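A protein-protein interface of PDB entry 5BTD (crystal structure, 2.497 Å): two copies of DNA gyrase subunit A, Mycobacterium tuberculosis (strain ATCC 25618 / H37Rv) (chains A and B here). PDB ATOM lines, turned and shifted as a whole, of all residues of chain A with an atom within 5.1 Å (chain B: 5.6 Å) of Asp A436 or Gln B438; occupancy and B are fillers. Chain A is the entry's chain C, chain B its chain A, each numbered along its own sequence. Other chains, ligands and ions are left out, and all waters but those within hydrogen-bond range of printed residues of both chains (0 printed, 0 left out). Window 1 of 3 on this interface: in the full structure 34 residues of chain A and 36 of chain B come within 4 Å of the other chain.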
ATOM      1  N   GLN A 432     -12.597   7.596  15.784  1.00  0.00           N
ATOM      2  CA  GLN A 432     -14.000   7.372  15.458  1.00  0.00           C
ATOM      3  C   GLN A 432     -14.280   5.879  15.322  1.00  0.00           C
ATOM      4  O   GLN A 432     -15.359   5.402  15.676  1.00  0.00           O
ATOM      5  CB  GLN A 432     -14.374   8.095  14.163  1.00  0.00           C
ATOM      6  CG  GLN A 432     -15.871   8.211  13.921  1.00  0.00           C
ATOM      7  CD  GLN A 432     -16.550   9.102  14.945  1.00  0.00           C
ATOM      8  OE1 GLN A 432     -17.079   8.625  15.950  1.00  0.00           O
ATOM      9  NE2 GLN A 432     -16.532  10.408  14.696  1.00  0.00           N
ATOM     10  N   ALA A 433     -13.301   5.148  14.797  1.00  0.00           N
ATOM     11  CA  ALA A 433     -13.438   3.710  14.597  1.00  0.00           C
ATOM     12  C   ALA A 433     -13.480   2.984  15.934  1.00  0.00           C
ATOM     13  O   ALA A 433     -14.241   2.029  16.103  1.00  0.00           O
ATOM     14  CB  ALA A 433     -12.298   3.181  13.745  1.00  0.00           C
ATOM     15  N   ILE A 434     -12.661   3.438  16.877  1.00  0.00           N
ATOM     16  CA  ILE A 434     -12.669   2.883  18.225  1.00  0.00           C
ATOM     17  C   ILE A 434     -14.054   3.070  18.830  1.00  0.00           C
ATOM     18  O   ILE A 434     -14.612   2.150  19.428  1.00  0.00           O
ATOM     19  CB  ILE A 434     -11.611   3.553  19.128  1.00  0.00           C
ATOM     20  CG1 ILE A 434     -10.207   3.331  18.563  1.00  0.00           C
ATOM     21  CG2 ILE A 434     -11.698   3.017  20.558  1.00  0.00           C
ATOM     22  CD1 ILE A 434      -9.145   4.202  19.205  1.00  0.00           C
ATOM     23  N   LEU A 435     -14.609   4.266  18.660  1.00  0.00           N
ATOM     24  CA  LEU A 435     -15.937   4.575  19.171  1.00  0.00           C
ATOM     25  C   LEU A 435     -16.992   3.697  18.495  1.00  0.00           C
ATOM     26  O   LEU A 435     -17.914   3.210  19.152  1.00  0.00           O
ATOM     27  CB  LEU A 435     -16.255   6.058  18.963  1.00  0.00           C
ATOM     28  CG  LEU A 435     -15.594   7.032  19.946  1.00  0.00           C
ATOM     29  CD1 LEU A 435     -15.803   8.471  19.495  1.00  0.00           C
ATOM     30  CD2 LEU A 435     -16.117   6.842  21.366  1.00  0.00           C
ATOM     31  N   ASP A 436     -16.845   3.486  17.188  1.00  0.00           N
ATOM     32  CA  ASP A 436     -17.793   2.672  16.426  1.00  0.00           C
ATOM     33  C   ASP A 436     -17.596   1.178  16.665  1.00  0.00           C
ATOM     34  O   ASP A 436     -18.367   0.358  16.170  1.00  0.00           O
ATOM     35  CB  ASP A 436     -17.667   2.954  14.925  1.00  0.00           C
ATOM     36  CG  ASP A 436     -18.101   4.357  14.551  1.00  0.00           C
ATOM     37  OD1 ASP A 436     -18.947   4.933  15.265  1.00  0.00           O
ATOM     38  OD2 ASP A 436     -17.604   4.877  13.528  1.00  0.00           O
ATOM     39  N   MET A 437     -16.563   0.829  17.423  1.00  0.00           N
ATOM     40  CA  MET A 437     -16.246  -0.569  17.678  1.00  0.00           C
ATOM     41  C   MET A 437     -17.330  -1.211  18.544  1.00  0.00           C
ATOM     42  O   MET A 437     -17.828  -0.592  19.484  1.00  0.00           O
ATOM     43  CB  MET A 437     -14.879  -0.682  18.356  1.00  0.00           C
ATOM     44  CG  MET A 437     -14.185  -2.015  18.150  1.00  0.00           C
ATOM     45  SD  MET A 437     -12.789  -2.290  19.262  1.00  0.00           S
ATOM     46  CE  MET A 437     -12.030  -0.666  19.311  1.00  0.00           C
ATOM     47  N   GLN A 438     -17.699  -2.447  18.217  1.00  0.00           N
ATOM     48  CA  GLN A 438     -18.710  -3.178  18.978  1.00  0.00           C
ATOM     49  C   GLN A 438     -18.086  -3.906  20.164  1.00  0.00           C
ATOM     50  O   GLN A 438     -16.896  -4.221  20.146  1.00  0.00           O
ATOM     51  CB  GLN A 438     -19.429  -4.185  18.084  1.00  0.00           C
ATOM     52  CG  GLN A 438     -20.293  -3.563  17.006  1.00  0.00           C
ATOM     53  CD  GLN A 438     -20.929  -4.607  16.103  1.00  0.00           C
ATOM     54  OE1 GLN A 438     -20.243  -5.469  15.553  1.00  0.00           O
ATOM     55  NE2 GLN A 438     -22.247  -4.538  15.953  1.00  0.00           N
ATOM     56  N   LEU A 439     -18.891  -4.173  21.191  1.00  0.00           N
ATOM     57  CA  LEU A 439     -18.423  -4.931  22.350  1.00  0.00           C
ATOM     58  C   LEU A 439     -18.031  -6.348  21.948  1.00  0.00           C
ATOM     59  O   LEU A 439     -17.233  -6.994  22.625  1.00  0.00           O
ATOM     60  CB  LEU A 439     -19.498  -4.975  23.441  1.00  0.00           C
ATOM     61  CG  LEU A 439     -19.896  -3.636  24.071  1.00  0.00           C
ATOM     62  CD1 LEU A 439     -20.959  -3.849  25.136  1.00  0.00           C
ATOM     63  CD2 LEU A 439     -18.692  -2.918  24.664  1.00  0.00           C
ATOM     64  N   ASP B 436     -23.889  -6.440  20.090  1.00  0.00           N
ATOM     65  CA  ASP B 436     -23.834  -5.559  18.930  1.00  0.00           C
ATOM     66  C   ASP B 436     -23.673  -4.093  19.330  1.00  0.00           C
ATOM     67  O   ASP B 436     -23.519  -3.226  18.472  1.00  0.00           O
ATOM     68  CB  ASP B 436     -25.097  -5.724  18.079  1.00  0.00           C
ATOM     69  CG  ASP B 436     -25.211  -7.104  17.458  1.00  0.00           C
ATOM     70  OD1 ASP B 436     -24.163  -7.748  17.229  1.00  0.00           O
ATOM     71  OD2 ASP B 436     -26.352  -7.541  17.191  1.00  0.00           O
ATOM     72  N   MET B 437     -23.705  -3.816  20.630  1.00  0.00           N
ATOM     73  CA  MET B 437     -23.615  -2.442  21.111  1.00  0.00           C
ATOM     74  C   MET B 437     -22.234  -1.849  20.858  1.00  0.00           C
ATOM     75  O   MET B 437     -21.217  -2.508  21.068  1.00  0.00           O
ATOM     76  CB  MET B 437     -23.925  -2.375  22.604  1.00  0.00           C
ATOM     77  CG  MET B 437     -24.414  -1.017  23.065  1.00  0.00           C
ATOM     78  SD  MET B 437     -24.378  -0.800  24.855  1.00  0.00           S
ATOM     79  CE  MET B 437     -24.908  -2.414  25.429  1.00  0.00           C
ATOM     80  N   GLN B 438     -22.210  -0.595  20.420  1.00  0.00           N
ATOM     81  CA  GLN B 438     -20.959   0.105  20.157  1.00  0.00           C
ATOM     82  C   GLN B 438     -20.436   0.784  21.415  1.00  0.00           C
ATOM     83  O   GLN B 438     -21.209   1.114  22.317  1.00  0.00           O
ATOM     84  CB  GLN B 438     -21.153   1.144  19.053  1.00  0.00           C
ATOM     85  CG  GLN B 438     -21.441   0.552  17.688  1.00  0.00           C
ATOM     86  CD  GLN B 438     -21.710   1.616  16.647  1.00  0.00           C
ATOM     87  OE1 GLN B 438     -22.557   2.489  16.842  1.00  0.00           O
ATOM     88  NE2 GLN B 438     -20.984   1.556  15.535  1.00  0.00           N
ATOM     89  N   LEU B 439     -19.125   1.000  21.466  1.00  0.00           N
ATOM     90  CA  LEU B 439     -18.506   1.711  22.581  1.00  0.00           C
ATOM     91  C   LEU B 439     -19.010   3.152  22.657  1.00  0.00           C
ATOM     92  O   LEU B 439     -18.928   3.788  23.708  1.00  0.00           O
ATOM     93  CB  LEU B 439     -16.980   1.693  22.457  1.00  0.00           C
ATOM     94  CG  LEU B 439     -16.302   0.321  22.527  1.00  0.00           C
ATOM     95  CD1 LEU B 439     -14.796   0.466  22.410  1.00  0.00           C
ATOM     96  CD2 LEU B 439     -16.661  -0.414  23.809  1.00  0.00           C
ATOM     97  N   ARG B 440     -19.520   3.654  21.534  1.00  0.00           N
ATOM     98  CA  ARG B 440     -20.136   4.977  21.470  1.00  0.00           C
ATOM     99  C   ARG B 440     -21.145   5.195  22.590  1.00  0.00           C
ATOM    100  O   ARG B 440     -21.150   6.240  23.239  1.00  0.00           O
ATOM    101  CB  ARG B 440     -20.848   5.162  20.127  1.00  0.00           C
ATOM    102  CG  ARG B 440     -20.024   5.820  19.048  1.00  0.00           C
ATOM    103  CD  ARG B 440     -20.838   5.996  17.778  1.00  0.00           C
ATOM    104  NE  ARG B 440     -20.139   6.813  16.790  1.00  0.00           N
ATOM    105  CZ  ARG B 440     -20.125   8.144  16.782  1.00  0.00           C
ATOM    106  NH1 ARG B 440     -20.776   8.833  17.711  1.00  0.00           N
ATOM    107  NH2 ARG B 440     -19.455   8.789  15.837  1.00  0.00           N
ATOM    108  N   ARG B 441     -21.997   4.199  22.806  1.00  0.00           N
ATOM    109  CA  ARG B 441     -23.115   4.336  23.731  1.00  0.00           C
ATOM    110  C   ARG B 441     -22.729   4.211  25.207  1.00  0.00           C
ATOM    111  O   ARG B 441     -23.595   4.291  26.079  1.00  0.00           O
ATOM    112  CB  ARG B 441     -24.210   3.323  23.386  1.00  0.00           C
ATOM    113  CG  ARG B 441     -24.993   3.708  22.136  1.00  0.00           C
ATOM    114  CD  ARG B 441     -26.188   2.803  21.889  1.00  0.00           C
ATOM    115  NE  ARG B 441     -25.836   1.606  21.133  1.00  0.00           N
ATOM    116  CZ  ARG B 441     -26.724   0.744  20.645  1.00  0.00           C
ATOM    117  NH1 ARG B 441     -28.023   0.944  20.834  1.00  0.00           N
ATOM    118  NH2 ARG B 441     -26.311  -0.317  19.967  1.00  0.00           N
ATOM    119  N   LEU B 442     -21.441   4.034  25.489  1.00  0.00           N
ATOM    120  CA  LEU B 442     -20.975   3.923  26.869  1.00  0.00           C
ATOM    121  C   LEU B 442     -20.663   5.299  27.459  1.00  0.00           C
ATOM    122  O   LEU B 442     -20.338   5.416  28.643  1.00  0.00           O
ATOM    123  CB  LEU B 442     -19.738   3.023  26.954  1.00  0.00           C
ATOM    124  CG  LEU B 442     -19.922   1.554  26.559  1.00  0.00           C
ATOM    125  CD1 LEU B 442     -18.623   0.788  26.747  1.00  0.00           C
ATOM    126  CD2 LEU B 442     -21.045   0.890  27.347  1.00  0.00           C
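Ile A434 touches Leu B439 (O to CD1, 3.4 Å). CB of Gln B438 touches O of Leu A435, at 3.8 Å. Gln B438 touches Met A437 (CA to O, 3.3 Å). O of Met B437 touches CA of Gln A438 (3.3 Å). Leu A439 touches Leu B439 (CD2 to CD2, 3.3 Å).
The backbone carbonyl oxygen (O) of Asp B436 is in hydrogen-bond range of the side-chain amide nitrogen (NE2) of Gln A438 (3.1 Å). O of Met B437 sits at hydrogen-bond distance from N of Leu A439 (2.9 Å). NE2 of Gln B438 sits at hydrogen-bond distance from O of Asp A436 (2.9 Å). The backbone NH (N) of Leu B439 lies within hydrogen-bond range of the backbone carbonyl oxygen (O) of Leu A435 (3.4 Å). The backbone NH of Leu B439 is in hydrogen-bond range of the backbone carbonyl oxygen of Met A437. The backbone NH (N) of Arg B440 lies within hydrogen-bond range of the backbone carbonyl oxygen (O) of Leu A435 (2.9 Å). The guanidinium group of Arg B440 is in salt-bridge range of the side-chain carboxylate of Asp A436. NH2 of Arg B440 lies close to OE1 of Gln A432 (2.4 Å).
Of the printed residues of chain B, Asp A436 touches Gln B438 (2.9 Å) and Arg B440 (2.7 Å). Of chain A, only Leu A435, Asp A436 and Met A437 come within 4 Å of Gln B438. Printed residues of chain B within 4 Å of Leu A435: Gln B438 (3.8 Å), Leu B439 (3.4 Å) and Arg B440 (2.9 Å). Printed residues of chain A within 4 Å of Asp B436: Gln A438 (3.1 Å). Of the printed residues of chain B, Leu A439 touches Met B437 and Leu B439. The nearest residue of chain B that does not touch Asp A436 is Leu B439 (5.0 Å).
Of the 7 printed residues of chain B, 5 touch a printed residue of chain A. Hydrophobic or aromatic side chains of chain B that line the printed part of chain A: Leu B439. Among the printed residues, 13 pairs touch across the chains. Among the printed residues, Asp or Glu carboxylates within 4 Å of a Lys or Arg side-chain nitrogen of the other chain: Asp A436 with Arg B440 (2.7 Å).
Asp A436 touches Gln B438, and with the chains exchanged Gln A438 touches Asp B436. Met A437 touches Gln B438, and with the chains exchanged Gln A438 touches Met B437. Met A437 touches Leu B439, and with the chains exchanged Leu A439 touches Met B437. Leu B439 touches its own counterpart, Leu A439. 4 positions are printed for both chains. Of the 13 pairs that touch across the chains among the printed residues, 7 have their exchanged pair printed and touching as well.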
